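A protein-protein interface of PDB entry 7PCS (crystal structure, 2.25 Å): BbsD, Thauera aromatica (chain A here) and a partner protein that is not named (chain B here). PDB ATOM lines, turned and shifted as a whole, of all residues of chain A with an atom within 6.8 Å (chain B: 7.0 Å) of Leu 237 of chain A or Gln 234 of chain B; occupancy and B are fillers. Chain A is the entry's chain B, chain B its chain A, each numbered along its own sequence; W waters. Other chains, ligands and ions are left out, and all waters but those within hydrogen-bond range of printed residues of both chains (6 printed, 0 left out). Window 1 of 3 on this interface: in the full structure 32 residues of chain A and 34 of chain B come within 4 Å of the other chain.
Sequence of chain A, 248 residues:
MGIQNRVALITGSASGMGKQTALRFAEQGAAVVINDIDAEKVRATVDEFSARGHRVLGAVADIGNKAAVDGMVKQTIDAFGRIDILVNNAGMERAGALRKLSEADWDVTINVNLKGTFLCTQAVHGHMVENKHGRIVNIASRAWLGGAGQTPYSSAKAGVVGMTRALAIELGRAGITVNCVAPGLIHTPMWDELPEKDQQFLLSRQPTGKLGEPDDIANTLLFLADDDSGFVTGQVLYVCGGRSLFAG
O of Tyr 230 of chain B lies within hydrogen-bond range of N of Gly 241 of chain A, 2.8 Å away. O of Cys 240 of chain A is in hydrogen-bond range of OH of Tyr 230 of chain B. OE1 of Gln 234 of chain B is in hydrogen-bond range of N of Tyr 238 of chain A.
The backbone carbonyl oxygen (O) of Val 180 of chain B sits at hydrogen-bond distance from the backbone NH (N) of Gly 233 of chain B (2.8 Å). OD1 of Asn 181 of chain B sits at hydrogen-bond distance from N of Gly 233 of chain B, at 3.2 Å. The side-chain hydroxyl (OG) of Ser 244 of chain A sits at hydrogen-bond distance from the side-chain sulfur (SG) of Cys 240 of chain A (2.9 Å). The backbone NH of Val 180 of chain B lies within hydrogen-bond range of the side-chain hydroxyl of Thr 232 of chain B, at 3.0 Å. The backbone NH of Ala 182 of chain A is in hydrogen-bond range of the backbone carbonyl oxygen of Leu 237 of chain A (3.0 Å). The backbone NH of Gln 234 of chain B is in hydrogen-bond range of the side-chain amide oxygen of Asn 181 of chain B (3.0 Å).
CA of Thr 220 of chain A touches CZ of Phe 222 of chain B, 3.9 Å away. Val 231 of chain B touches Thr 220 of chain A (CG2 to OG1, 3.9 Å). Phe 222 of chain B touches Phe 223 of chain A. Leu 236 of chain B touches Gln 235 of chain A (CD1 to CG, 3.9 Å). C of Leu 237 of chain A touches OE1 of Gln 234 of chain B (3.9 Å). Val 231 of chain B touches Tyr 238 of chain A (CG1 to O, 3.8 Å). Tyr 230 of chain B touches Val 239 of chain A. Gly 241 of chain A touches Thr 232 of chain B (C to CG2, 3.8 Å). Arg 167 of chain B touches Leu 245 of chain A. Leu 245 of chain A touches Gly 233 of chain B.
Leu 237 of chain A touches just one residue of chain B: Gln 234. Of the printed residues of chain B, Cys 240 of chain A touches Tyr 230. Of the printed residues of chain B, Gly 242 of chain A touches Thr 232. Of the printed residues of chain B, Leu 245 of chain A touches Arg 167 and Gly 233. Asn 140 of chain B touches none of the printed residues of chain A. Printed residues of chain A within 4 Å of Arg 167 of chain B: Leu 245. Of the printed residues of chain A, Thr 232 of chain B touches Gly 241 (3.8 Å) and Gly 242 (3.5 Å). Of the printed residues of chain A, Gln 234 of chain B touches Leu 237 and Tyr 238. The nearest residue of chain B that does not touch Leu 237 of chain A is Phe 222 of chain B (4.02 Å). The nearest printed residue of chain B that does not touch Val 239 of chain A is Val 231 of chain B (4.4 Å).
Hydrophobic or aromatic side chains of chain B within 4 Å of the printed part of chain A: Phe 222, Tyr 230, Val 231 and Leu 236. Of the 18 printed residues of chain A, 10 touch a printed residue of chain B. Hydrophobic or aromatic side chains of chain A that line the printed part of chain B: Phe 223, Leu 237, Tyr 238, Val 239 and Leu 245. Among the printed residues, 15 pairs touch across the chains.
Water W1 lies within hydrogen-bond range of O of Val 236 of chain A (2.7 Å) and O of Thr 235 of chain B (3.2 Å). Water W2 lies within hydrogen-bond range of the backbone carbonyl oxygen of Cys 240 of chain A (2.7 Å) and the side-chain hydroxyl of Tyr 230 of chain B (3.2 Å). Water W6 lies within hydrogen-bond range of OE1 of Gln 234 of chain B (2.7 Å), N of Thr 235 of chain B (3.1 Å) and O of Val 236 of chain A (3.5 Å). Water W5 lies within hydrogen-bond range of OG of Ser 244 of chain A (2.7 Å) and NE2 of Gln 234 of chain B (3.3 Å). Water W4 lies within hydrogen-bond range of the backbone carbonyl oxygen of Tyr 238 of chain A (2.8 Å), the side-chain sulfur of Cys 240 of chain A (3.1 Å), the backbone NH of Thr 232 of chain B (3.2 Å), the side-chain amide nitrogen of Gln 234 of chain B (3.3 Å) and the backbone carbonyl oxygen of Tyr 230 of chain B (3.4 Å). Water W3 lies within hydrogen-bond range of the backbone carbonyl oxygen of Leu 245 of chain A (3.0 Å) and the guanidinium group of Arg 167 of chain B (3.0 Å).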
ATOM      1  N   ASN A 179      -6.388 -31.515  16.276  1.00  0.00           N
ATOM      2  CA  ASN A 179      -7.370 -30.497  15.950  1.00  0.00           C
ATOM      3  C   ASN A 179      -7.796 -29.777  17.219  1.00  0.00           C
ATOM      4  O   ASN A 179      -7.494 -30.202  18.336  1.00  0.00           O
ATOM      5  CB  ASN A 179      -8.593 -31.102  15.249  1.00  0.00           C
ATOM      6  CG  ASN A 179      -8.279 -31.590  13.846  1.00  0.00           C
ATOM      7  OD1 ASN A 179      -8.043 -30.787  12.941  1.00  0.00           O
ATOM      8  ND2 ASN A 179      -8.280 -32.916  13.657  1.00  0.00           N
ATOM      9  N   CYS A 180      -8.538 -28.693  17.033  1.00  0.00           N
ATOM     10  CA  CYS A 180      -8.967 -27.851  18.134  1.00  0.00           C
ATOM     11  C   CYS A 180     -10.425 -27.472  17.928  1.00  0.00           C
ATOM     12  O   CYS A 180     -10.836 -27.130  16.815  1.00  0.00           O
ATOM     13  CB  CYS A 180      -8.094 -26.609  18.219  1.00  0.00           C
ATOM     14  SG  CYS A 180      -8.652 -25.506  19.468  1.00  0.00           S
ATOM     15  N   VAL A 181     -11.206 -27.554  19.000  1.00  0.00           N
ATOM     16  CA  VAL A 181     -12.589 -27.097  19.006  1.00  0.00           C
ATOM     17  C   VAL A 181     -12.672 -25.890  19.930  1.00  0.00           C
ATOM     18  O   VAL A 181     -12.227 -25.953  21.084  1.00  0.00           O
ATOM     19  CB  VAL A 181     -13.553 -28.211  19.444  1.00  0.00           C
ATOM     20  CG1 VAL A 181     -14.915 -27.618  19.773  1.00  0.00           C
ATOM     21  CG2 VAL A 181     -13.676 -29.256  18.352  1.00  0.00           C
ATOM     22  N   ALA A 182     -13.228 -24.788  19.422  1.00  0.00           N
ATOM     23  CA  ALA A 182     -13.356 -23.541  20.170  1.00  0.00           C
ATOM     24  C   ALA A 182     -14.829 -23.298  20.454  1.00  0.00           C
ATOM     25  O   ALA A 182     -15.540 -22.708  19.624  1.00  0.00           O
ATOM     26  CB  ALA A 182     -12.753 -22.369  19.395  1.00  0.00           C
ATOM     27  N   PRO A 183     -15.345 -23.750  21.593  1.00  0.00           N
ATOM     28  CA  PRO A 183     -16.771 -23.549  21.878  1.00  0.00           C
ATOM     29  C   PRO A 183     -17.078 -22.084  22.117  1.00  0.00           C
ATOM     30  O   PRO A 183     -16.310 -21.365  22.760  1.00  0.00           O
ATOM     31  CB  PRO A 183     -17.016 -24.376  23.148  1.00  0.00           C
ATOM     32  CG  PRO A 183     -15.822 -25.265  23.284  1.00  0.00           C
ATOM     33  CD  PRO A 183     -14.671 -24.505  22.661  1.00  0.00           C
ATOM     34  N   THR A 220     -19.497 -32.554  17.387  1.00  0.00           N
ATOM     35  CA  THR A 220     -18.349 -32.046  16.646  1.00  0.00           C
ATOM     36  C   THR A 220     -17.099 -32.858  16.953  1.00  0.00           C
ATOM     37  O   THR A 220     -16.318 -33.167  16.047  1.00  0.00           O
ATOM     38  CB  THR A 220     -18.123 -30.574  16.978  1.00  0.00           C
ATOM     39  OG1 THR A 220     -19.335 -29.852  16.742  1.00  0.00           O
ATOM     40  CG2 THR A 220     -16.989 -29.996  16.124  1.00  0.00           C
ATOM     41  N   PHE A 223     -16.958 -36.155  15.159  1.00  0.00           N
ATOM     42  CA  PHE A 223     -16.507 -36.030  13.780  1.00  0.00           C
ATOM     43  C   PHE A 223     -14.986 -36.000  13.699  1.00  0.00           C
ATOM     44  O   PHE A 223     -14.382 -36.736  12.912  1.00  0.00           O
ATOM     45  CB  PHE A 223     -17.095 -34.779  13.146  1.00  0.00           C
ATOM     46  CG  PHE A 223     -16.361 -34.326  11.925  1.00  0.00           C
ATOM     47  CD1 PHE A 223     -16.331 -35.115  10.788  1.00  0.00           C
ATOM     48  CD2 PHE A 223     -15.702 -33.113  11.907  1.00  0.00           C
ATOM     49  CE1 PHE A 223     -15.665 -34.702   9.650  1.00  0.00           C
ATOM     50  CE2 PHE A 223     -15.031 -32.693  10.765  1.00  0.00           C
ATOM     51  CZ  PHE A 223     -15.017 -33.491   9.637  1.00  0.00           C
ATOM     52  N   LEU A 224     -14.347 -35.150  14.504  1.00  0.00           N
ATOM     53  CA  LEU A 224     -12.895 -35.013  14.436  1.00  0.00           C
ATOM     54  C   LEU A 224     -12.185 -36.296  14.848  1.00  0.00           C
ATOM     55  O   LEU A 224     -11.093 -36.592  14.347  1.00  0.00           O
ATOM     56  CB  LEU A 224     -12.438 -33.863  15.332  1.00  0.00           C
ATOM     57  CG  LEU A 224     -12.929 -32.466  14.956  1.00  0.00           C
ATOM     58  CD1 LEU A 224     -12.560 -31.434  16.011  1.00  0.00           C
ATOM     59  CD2 LEU A 224     -12.324 -32.101  13.605  1.00  0.00           C
ATOM     60  N   GLN A 235      -6.793 -27.953  12.473  1.00  0.00           N
ATOM     61  CA  GLN A 235      -7.964 -27.106  12.321  1.00  0.00           C
ATOM     62  C   GLN A 235      -8.403 -26.499  13.648  1.00  0.00           C
ATOM     63  O   GLN A 235      -8.217 -27.079  14.722  1.00  0.00           O
ATOM     64  CB  GLN A 235      -9.131 -27.891  11.719  1.00  0.00           C
ATOM     65  CG  GLN A 235      -8.858 -28.426  10.346  1.00  0.00           C
ATOM     66  CD  GLN A 235      -8.398 -27.358   9.400  1.00  0.00           C
ATOM     67  OE1 GLN A 235      -9.167 -26.475   9.027  1.00  0.00           O
ATOM     68  NE2 GLN A 235      -7.134 -27.422   9.010  1.00  0.00           N
ATOM     69  N   VAL A 236      -8.983 -25.307  13.553  1.00  0.00           N
ATOM     70  CA  VAL A 236      -9.681 -24.658  14.656  1.00  0.00           C
ATOM     71  C   VAL A 236     -11.135 -24.521  14.222  1.00  0.00           C
ATOM     72  O   VAL A 236     -11.457 -23.684  13.370  1.00  0.00           O
ATOM     73  CB  VAL A 236      -9.074 -23.294  15.006  1.00  0.00           C
ATOM     74  CG1 VAL A 236      -9.878 -22.643  16.115  1.00  0.00           C
ATOM     75  CG2 VAL A 236      -7.617 -23.449  15.417  1.00  0.00           C
ATOM     76  N   LEU A 237     -12.008 -25.345  14.788  1.00  0.00           N
ATOM     77  CA  LEU A 237     -13.411 -25.395  14.404  1.00  0.00           C
ATOM     78  C   LEU A 237     -14.248 -24.827  15.537  1.00  0.00           C
ATOM     79  O   LEU A 237     -14.232 -25.358  16.653  1.00  0.00           O
ATOM     80  CB  LEU A 237     -13.819 -26.831  14.083  1.00  0.00           C
ATOM     81  CG  LEU A 237     -15.197 -27.056  13.473  1.00  0.00           C
ATOM     82  CD1 LEU A 237     -15.324 -26.378  12.126  1.00  0.00           C
ATOM     83  CD2 LEU A 237     -15.443 -28.565  13.357  1.00  0.00           C
ATOM     84  N   TYR A 238     -14.967 -23.748  15.253  1.00  0.00           N
ATOM     85  CA  TYR A 238     -15.785 -23.087  16.254  1.00  0.00           C
ATOM     86  C   TYR A 238     -17.149 -23.757  16.345  1.00  0.00           C
ATOM     87  O   TYR A 238     -17.764 -24.083  15.327  1.00  0.00           O
ATOM     88  CB  TYR A 238     -15.953 -21.603  15.916  1.00  0.00           C
ATOM     89  CG  TYR A 238     -14.662 -20.806  15.902  1.00  0.00           C
ATOM     90  CD1 TYR A 238     -13.898 -20.701  14.746  1.00  0.00           C
ATOM     91  CD2 TYR A 238     -14.214 -20.148  17.044  1.00  0.00           C
ATOM     92  CE1 TYR A 238     -12.724 -19.965  14.732  1.00  0.00           C
ATOM     93  CE2 TYR A 238     -13.046 -19.417  17.040  1.00  0.00           C
ATOM     94  CZ  TYR A 238     -12.306 -19.328  15.881  1.00  0.00           C
ATOM     95  OH  TYR A 238     -11.144 -18.600  15.882  1.00  0.00           O
ATOM     96  N   VAL A 239     -17.606 -23.970  17.575  1.00  0.00           N
ATOM     97  CA  VAL A 239     -18.947 -24.459  17.864  1.00  0.00           C
ATOM     98  C   VAL A 239     -19.620 -23.334  18.635  1.00  0.00           C
ATOM     99  O   VAL A 239     -19.718 -23.377  19.866  1.00  0.00           O
ATOM    100  CB  VAL A 239     -18.913 -25.778  18.653  1.00  0.00           C
ATOM    101  CG1 VAL A 239     -20.318 -26.286  18.852  1.00  0.00           C
ATOM    102  CG2 VAL A 239     -18.080 -26.794  17.888  1.00  0.00           C
ATOM    103  N   CYS A 240     -20.071 -22.308  17.908  1.00  0.00           N
ATOM    104  CA  CYS A 240     -20.495 -21.056  18.516  1.00  0.00           C
ATOM    105  C   CYS A 240     -21.856 -20.556  18.058  1.00  0.00           C
ATOM    106  O   CYS A 240     -22.344 -19.565  18.616  1.00  0.00           O
ATOM    107  CB  CYS A 240     -19.467 -19.956  18.219  1.00  0.00           C
ATOM    108  SG  CYS A 240     -19.281 -19.641  16.428  1.00  0.00           S
ATOM    109  N   GLY A 241     -22.477 -21.183  17.064  1.00  0.00           N
ATOM    110  CA  GLY A 241     -23.708 -20.635  16.538  1.00  0.00           C
ATOM    111  C   GLY A 241     -23.521 -19.319  15.825  1.00  0.00           C
ATOM    112  O   GLY A 241     -24.465 -18.530  15.735  1.00  0.00           O
ATOM    113  N   GLY A 242     -22.316 -19.056  15.326  1.00  0.00           N
ATOM    114  CA  GLY A 242     -22.014 -17.839  14.613  1.00  0.00           C
ATOM    115  C   GLY A 242     -21.447 -16.716  15.453  1.00  0.00           C
ATOM    116  O   GLY A 242     -20.976 -15.722  14.887  1.00  0.00           O
ATOM    117  N   SER A 244     -18.709 -16.450  16.966  1.00  0.00           N
ATOM    118  CA  SER A 244     -17.294 -16.200  16.710  1.00  0.00           C
ATOM    119  C   SER A 244     -17.070 -15.320  15.486  1.00  0.00           C
ATOM    120  O   SER A 244     -16.007 -14.701  15.369  1.00  0.00           O
ATOM    121  CB  SER A 244     -16.548 -17.527  16.542  1.00  0.00           C
ATOM    122  OG  SER A 244     -16.988 -18.238  15.393  1.00  0.00           O
ATOM    123  N   LEU A 245     -18.043 -15.242  14.575  1.00  0.00           N
ATOM    124  CA  LEU A 245     -17.880 -14.390  13.399  1.00  0.00           C
ATOM    125  C   LEU A 245     -17.875 -12.915  13.781  1.00  0.00           C
ATOM    126  O   LEU A 245     -17.174 -12.116  13.151  1.00  0.00           O
ATOM    127  CB  LEU A 245     -18.977 -14.682  12.375  1.00  0.00           C
ATOM    128  CG  LEU A 245     -19.143 -16.163  12.024  1.00  0.00           C
ATOM    129  CD1 LEU A 245     -20.340 -16.361  11.090  1.00  0.00           C
ATOM    130  CD2 LEU A 245     -17.885 -16.745  11.419  1.00  0.00           C
ATOM    131  N   ASN B 140     -20.225 -24.718   1.073  1.00  0.00           N
ATOM    132  CA  ASN B 140     -19.440 -24.283  -0.072  1.00  0.00           C
ATOM    133  C   ASN B 140     -18.142 -25.073  -0.093  1.00  0.00           C
ATOM    134  O   ASN B 140     -17.476 -25.206   0.937  1.00  0.00           O
ATOM    135  CB  ASN B 140     -19.166 -22.781   0.025  1.00  0.00           C
ATOM    136  CG  ASN B 140     -18.164 -22.307  -0.986  1.00  0.00           C
ATOM    137  OD1 ASN B 140     -18.338 -22.482  -2.188  1.00  0.00           O
ATOM    138  ND2 ASN B 140     -17.110 -21.682  -0.505  1.00  0.00           N
ATOM    139  N   PHE B 163     -15.290 -16.444   1.049  1.00  0.00           N
ATOM    140  CA  PHE B 163     -15.031 -16.365   2.481  1.00  0.00           C
ATOM    141  C   PHE B 163     -15.994 -15.396   3.157  1.00  0.00           C
ATOM    142  O   PHE B 163     -16.762 -15.779   4.045  1.00  0.00           O
ATOM    143  CB  PHE B 163     -13.581 -15.936   2.713  1.00  0.00           C
ATOM    144  CG  PHE B 163     -13.265 -15.603   4.148  1.00  0.00           C
ATOM    145  CD1 PHE B 163     -13.142 -16.605   5.095  1.00  0.00           C
ATOM    146  CD2 PHE B 163     -13.091 -14.286   4.548  1.00  0.00           C
ATOM    147  CE1 PHE B 163     -12.849 -16.293   6.419  1.00  0.00           C
ATOM    148  CE2 PHE B 163     -12.811 -13.977   5.859  1.00  0.00           C
ATOM    149  CZ  PHE B 163     -12.695 -14.979   6.793  1.00  0.00           C
ATOM    150  N   THR B 166     -19.942 -16.379   2.472  1.00  0.00           N
ATOM    151  CA  THR B 166     -20.525 -17.414   3.319  1.00  0.00           C
ATOM    152  C   THR B 166     -20.768 -16.890   4.728  1.00  0.00           C
ATOM    153  O   THR B 166     -21.852 -17.080   5.294  1.00  0.00           O
ATOM    154  CB  THR B 166     -19.631 -18.655   3.353  1.00  0.00           C
ATOM    155  OG1 THR B 166     -18.294 -18.282   3.697  1.00  0.00           O
ATOM    156  CG2 THR B 166     -19.630 -19.352   2.009  1.00  0.00           C
ATOM    157  N   ARG B 167     -19.781 -16.191   5.297  1.00  0.00           N
ATOM    158  CA  ARG B 167     -19.910 -15.693   6.662  1.00  0.00           C
ATOM    159  C   ARG B 167     -20.982 -14.612   6.762  1.00  0.00           C
ATOM    160  O   ARG B 167     -21.711 -14.549   7.758  1.00  0.00           O
ATOM    161  CB  ARG B 167     -18.557 -15.171   7.142  1.00  0.00           C
ATOM    162  CG  ARG B 167     -17.523 -16.289   7.421  1.00  0.00           C
ATOM    163  CD  ARG B 167     -16.108 -15.743   7.412  1.00  0.00           C
ATOM    164  NE  ARG B 167     -15.948 -14.686   8.402  1.00  0.00           N
ATOM    165  CZ  ARG B 167     -15.321 -14.845   9.557  1.00  0.00           C
ATOM    166  NH1 ARG B 167     -14.754 -15.996   9.880  1.00  0.00           N
ATOM    167  NH2 ARG B 167     -15.262 -13.825  10.408  1.00  0.00           N
ATOM    168  N   ALA B 170     -24.188 -16.534   6.653  1.00  0.00           N
ATOM    169  CA  ALA B 170     -24.297 -17.288   7.894  1.00  0.00           C
ATOM    170  C   ALA B 170     -24.933 -16.432   8.978  1.00  0.00           C
ATOM    171  O   ALA B 170     -25.881 -16.852   9.653  1.00  0.00           O
ATOM    172  CB  ALA B 170     -22.918 -17.773   8.337  1.00  0.00           C
ATOM    173  N   VAL B 180     -24.325 -21.869   7.152  1.00  0.00           N
ATOM    174  CA  VAL B 180     -23.549 -21.726   5.926  1.00  0.00           C
ATOM    175  C   VAL B 180     -22.087 -21.923   6.292  1.00  0.00           C
ATOM    176  O   VAL B 180     -21.527 -21.128   7.055  1.00  0.00           O
ATOM    177  CB  VAL B 180     -23.757 -20.355   5.262  1.00  0.00           C
ATOM    178  CG1 VAL B 180     -23.098 -20.330   3.895  1.00  0.00           C
ATOM    179  CG2 VAL B 180     -25.241 -20.029   5.156  1.00  0.00           C
ATOM    180  N   ASN B 181     -21.471 -22.972   5.750  1.00  0.00           N
ATOM    181  CA  ASN B 181     -20.101 -23.336   6.076  1.00  0.00           C
ATOM    182  C   ASN B 181     -19.338 -23.597   4.785  1.00  0.00           C
ATOM    183  O   ASN B 181     -19.921 -23.718   3.705  1.00  0.00           O
ATOM    184  CB  ASN B 181     -20.053 -24.568   6.985  1.00  0.00           C
ATOM    185  CG  ASN B 181     -20.668 -24.304   8.347  1.00  0.00           C
ATOM    186  OD1 ASN B 181     -20.113 -23.567   9.159  1.00  0.00           O
ATOM    187  ND2 ASN B 181     -21.805 -24.930   8.613  1.00  0.00           N
ATOM    188  N   THR B 182     -18.017 -23.661   4.908  1.00  0.00           N
ATOM    189  CA  THR B 182     -17.125 -23.862   3.779  1.00  0.00           C
ATOM    190  C   THR B 182     -16.156 -24.994   4.080  1.00  0.00           C
ATOM    191  O   THR B 182     -15.502 -24.998   5.129  1.00  0.00           O
ATOM    192  CB  THR B 182     -16.337 -22.588   3.457  1.00  0.00           C
ATOM    193  OG1 THR B 182     -17.243 -21.527   3.125  1.00  0.00           O
ATOM    194  CG2 THR B 182     -15.364 -22.837   2.305  1.00  0.00           C
ATOM    195  N   VAL B 183     -16.075 -25.947   3.158  1.00  0.00           N
ATOM    196  CA  VAL B 183     -15.041 -26.972   3.155  1.00  0.00           C
ATOM    197  C   VAL B 183     -13.994 -26.561   2.127  1.00  0.00           C
ATOM    198  O   VAL B 183     -14.313 -26.392   0.944  1.00  0.00           O
ATOM    199  CB  VAL B 183     -15.616 -28.359   2.832  1.00  0.00           C
ATOM    200  CG1 VAL B 183     -14.477 -29.351   2.593  1.00  0.00           C
ATOM    201  CG2 VAL B 183     -16.526 -28.837   3.949  1.00  0.00           C
ATOM    202  N   VAL B 184     -12.756 -26.384   2.572  1.00  0.00           N
ATOM    203  CA  VAL B 184     -11.661 -25.972   1.701  1.00  0.00           C
ATOM    204  C   VAL B 184     -10.824 -27.199   1.398  1.00  0.00           C
ATOM    205  O   VAL B 184     -10.188 -27.761   2.296  1.00  0.00           O
ATOM    206  CB  VAL B 184     -10.807 -24.867   2.333  1.00  0.00           C
ATOM    207  CG1 VAL B 184      -9.698 -24.441   1.372  1.00  0.00           C
ATOM    208  CG2 VAL B 184     -11.684 -23.674   2.713  1.00  0.00           C
ATOM    209  N   PHE B 222     -20.519 -33.999   7.471  1.00  0.00           N
ATOM    210  CA  PHE B 222     -20.611 -33.535   8.849  1.00  0.00           C
ATOM    211  C   PHE B 222     -21.339 -32.202   8.927  1.00  0.00           C
ATOM    212  O   PHE B 222     -22.233 -32.013   9.761  1.00  0.00           O
ATOM    213  CB  PHE B 222     -19.225 -33.409   9.476  1.00  0.00           C
ATOM    214  CG  PHE B 222     -19.221 -32.565  10.722  1.00  0.00           C
ATOM    215  CD1 PHE B 222     -19.871 -32.999  11.867  1.00  0.00           C
ATOM    216  CD2 PHE B 222     -18.599 -31.331  10.742  1.00  0.00           C
ATOM    217  CE1 PHE B 222     -19.894 -32.224  13.009  1.00  0.00           C
ATOM    218  CE2 PHE B 222     -18.614 -30.551  11.885  1.00  0.00           C
ATOM    219  CZ  PHE B 222     -19.262 -30.999  13.020  1.00  0.00           C
ATOM    220  N   LEU B 223     -20.949 -31.249   8.085  1.00  0.00           N
ATOM    221  CA  LEU B 223     -21.562 -29.928   8.139  1.00  0.00           C
ATOM    222  C   LEU B 223     -23.035 -29.965   7.745  1.00  0.00           C
ATOM    223  O   LEU B 223     -23.823 -29.136   8.217  1.00  0.00           O
ATOM    224  CB  LEU B 223     -20.796 -28.965   7.234  1.00  0.00           C
ATOM    225  CG  LEU B 223     -19.305 -28.831   7.568  1.00  0.00           C
ATOM    226  CD1 LEU B 223     -18.564 -27.993   6.526  1.00  0.00           C
ATOM    227  CD2 LEU B 223     -19.108 -28.244   8.957  1.00  0.00           C
ATOM    228  N   TYR B 230     -25.275 -25.897  15.442  1.00  0.00           N
ATOM    229  CA  TYR B 230     -24.583 -24.820  16.142  1.00  0.00           C
ATOM    230  C   TYR B 230     -23.227 -24.507  15.517  1.00  0.00           C
ATOM    231  O   TYR B 230     -22.426 -23.782  16.118  1.00  0.00           O
ATOM    232  CB  TYR B 230     -24.410 -25.182  17.620  1.00  0.00           C
ATOM    233  CG  TYR B 230     -24.304 -23.985  18.545  1.00  0.00           C
ATOM    234  CD1 TYR B 230     -25.351 -23.075  18.668  1.00  0.00           C
ATOM    235  CD2 TYR B 230     -23.163 -23.775  19.309  1.00  0.00           C
ATOM    236  CE1 TYR B 230     -25.253 -21.987  19.516  1.00  0.00           C
ATOM    237  CE2 TYR B 230     -23.057 -22.692  20.159  1.00  0.00           C
ATOM    238  CZ  TYR B 230     -24.103 -21.801  20.259  1.00  0.00           C
ATOM    239  OH  TYR B 230     -23.997 -20.722  21.105  1.00  0.00           O
ATOM    240  N   VAL B 231     -22.952 -25.044  14.331  1.00  0.00           N
ATOM    241  CA  VAL B 231     -21.712 -24.805  13.599  1.00  0.00           C
ATOM    242  C   VAL B 231     -22.073 -24.025  12.344  1.00  0.00           C
ATOM    243  O   VAL B 231     -22.756 -24.545  11.452  1.00  0.00           O
ATOM    244  CB  VAL B 231     -21.001 -26.116  13.239  1.00  0.00           C
ATOM    245  CG1 VAL B 231     -19.678 -25.839  12.532  1.00  0.00           C
ATOM    246  CG2 VAL B 231     -20.786 -26.968  14.484  1.00  0.00           C
ATOM    247  N   THR B 232     -21.626 -22.777  12.267  1.00  0.00           N
ATOM    248  CA  THR B 232     -21.914 -21.966  11.098  1.00  0.00           C
ATOM    249  C   THR B 232     -20.808 -20.940  10.916  1.00  0.00           C
ATOM    250  O   THR B 232     -20.123 -20.558  11.869  1.00  0.00           O
ATOM    251  CB  THR B 232     -23.276 -21.270  11.209  1.00  0.00           C
ATOM    252  OG1 THR B 232     -23.729 -20.901   9.900  1.00  0.00           O
ATOM    253  CG2 THR B 232     -23.173 -20.021  12.077  1.00  0.00           C
ATOM    254  N   GLY B 233     -20.648 -20.499   9.668  1.00  0.00           N
ATOM    255  CA  GLY B 233     -19.634 -19.525   9.327  1.00  0.00           C
ATOM    256  C   GLY B 233     -18.227 -20.066   9.283  1.00  0.00           C
ATOM    257  O   GLY B 233     -17.280 -19.277   9.261  1.00  0.00           O
ATOM    258  N   GLN B 234     -18.060 -21.380   9.257  1.00  0.00           N
ATOM    259  CA  GLN B 234     -16.755 -21.994   9.426  1.00  0.00           C
ATOM    260  C   GLN B 234     -16.037 -22.184   8.095  1.00  0.00           C
ATOM    261  O   GLN B 234     -16.652 -22.396   7.048  1.00  0.00           O
ATOM    262  CB  GLN B 234     -16.897 -23.343  10.131  1.00  0.00           C
ATOM    263  CG  GLN B 234     -17.536 -23.250  11.492  1.00  0.00           C
ATOM    264  CD  GLN B 234     -16.814 -22.268  12.384  1.00  0.00           C
ATOM    265  OE1 GLN B 234     -15.695 -22.522  12.813  1.00  0.00           O
ATOM    266  NE2 GLN B 234     -17.446 -21.132  12.654  1.00  0.00           N
ATOM    267  N   THR B 235     -14.715 -22.097   8.158  1.00  0.00           N
ATOM    268  CA  THR B 235     -13.807 -22.370   7.051  1.00  0.00           C
ATOM    269  C   THR B 235     -13.008 -23.598   7.479  1.00  0.00           C
ATOM    270  O   THR B 235     -11.983 -23.491   8.160  1.00  0.00           O
ATOM    271  CB  THR B 235     -12.919 -21.167   6.766  1.00  0.00           C
ATOM    272  OG1 THR B 235     -13.733 -19.995   6.647  1.00  0.00           O
ATOM    273  CG2 THR B 235     -12.171 -21.354   5.463  1.00  0.00           C
ATOM    274  N   LEU B 236     -13.514 -24.775   7.119  1.00  0.00           N
ATOM    275  CA  LEU B 236     -12.933 -26.049   7.534  1.00  0.00           C
ATOM    276  C   LEU B 236     -12.039 -26.574   6.417  1.00  0.00           C
ATOM    277  O   LEU B 236     -12.523 -26.922   5.337  1.00  0.00           O
ATOM    278  CB  LEU B 236     -14.031 -27.058   7.874  1.00  0.00           C
ATOM    279  CG  LEU B 236     -13.561 -28.466   8.257  1.00  0.00           C
ATOM    280  CD1 LEU B 236     -12.629 -28.430   9.461  1.00  0.00           C
ATOM    281  CD2 LEU B 236     -14.748 -29.385   8.538  1.00  0.00           C
HETATM  282  O   HOH W   1     -12.450 -24.746  11.096  1.00  0.00           O
HETATM  283  O   HOH W   2     -21.817 -18.347  20.980  1.00  0.00           O
HETATM  284  O   HOH W   3     -17.634 -11.927  10.206  1.00  0.00           O
HETATM  285  O   HOH W   4     -19.720 -22.200  14.725  1.00  0.00           O
HETATM  286  O   HOH W   5     -15.403 -18.625  13.186  1.00  0.00           O
HETATM  287  O   HOH W   6     -13.664 -22.440  11.005  1.00  0.00           O
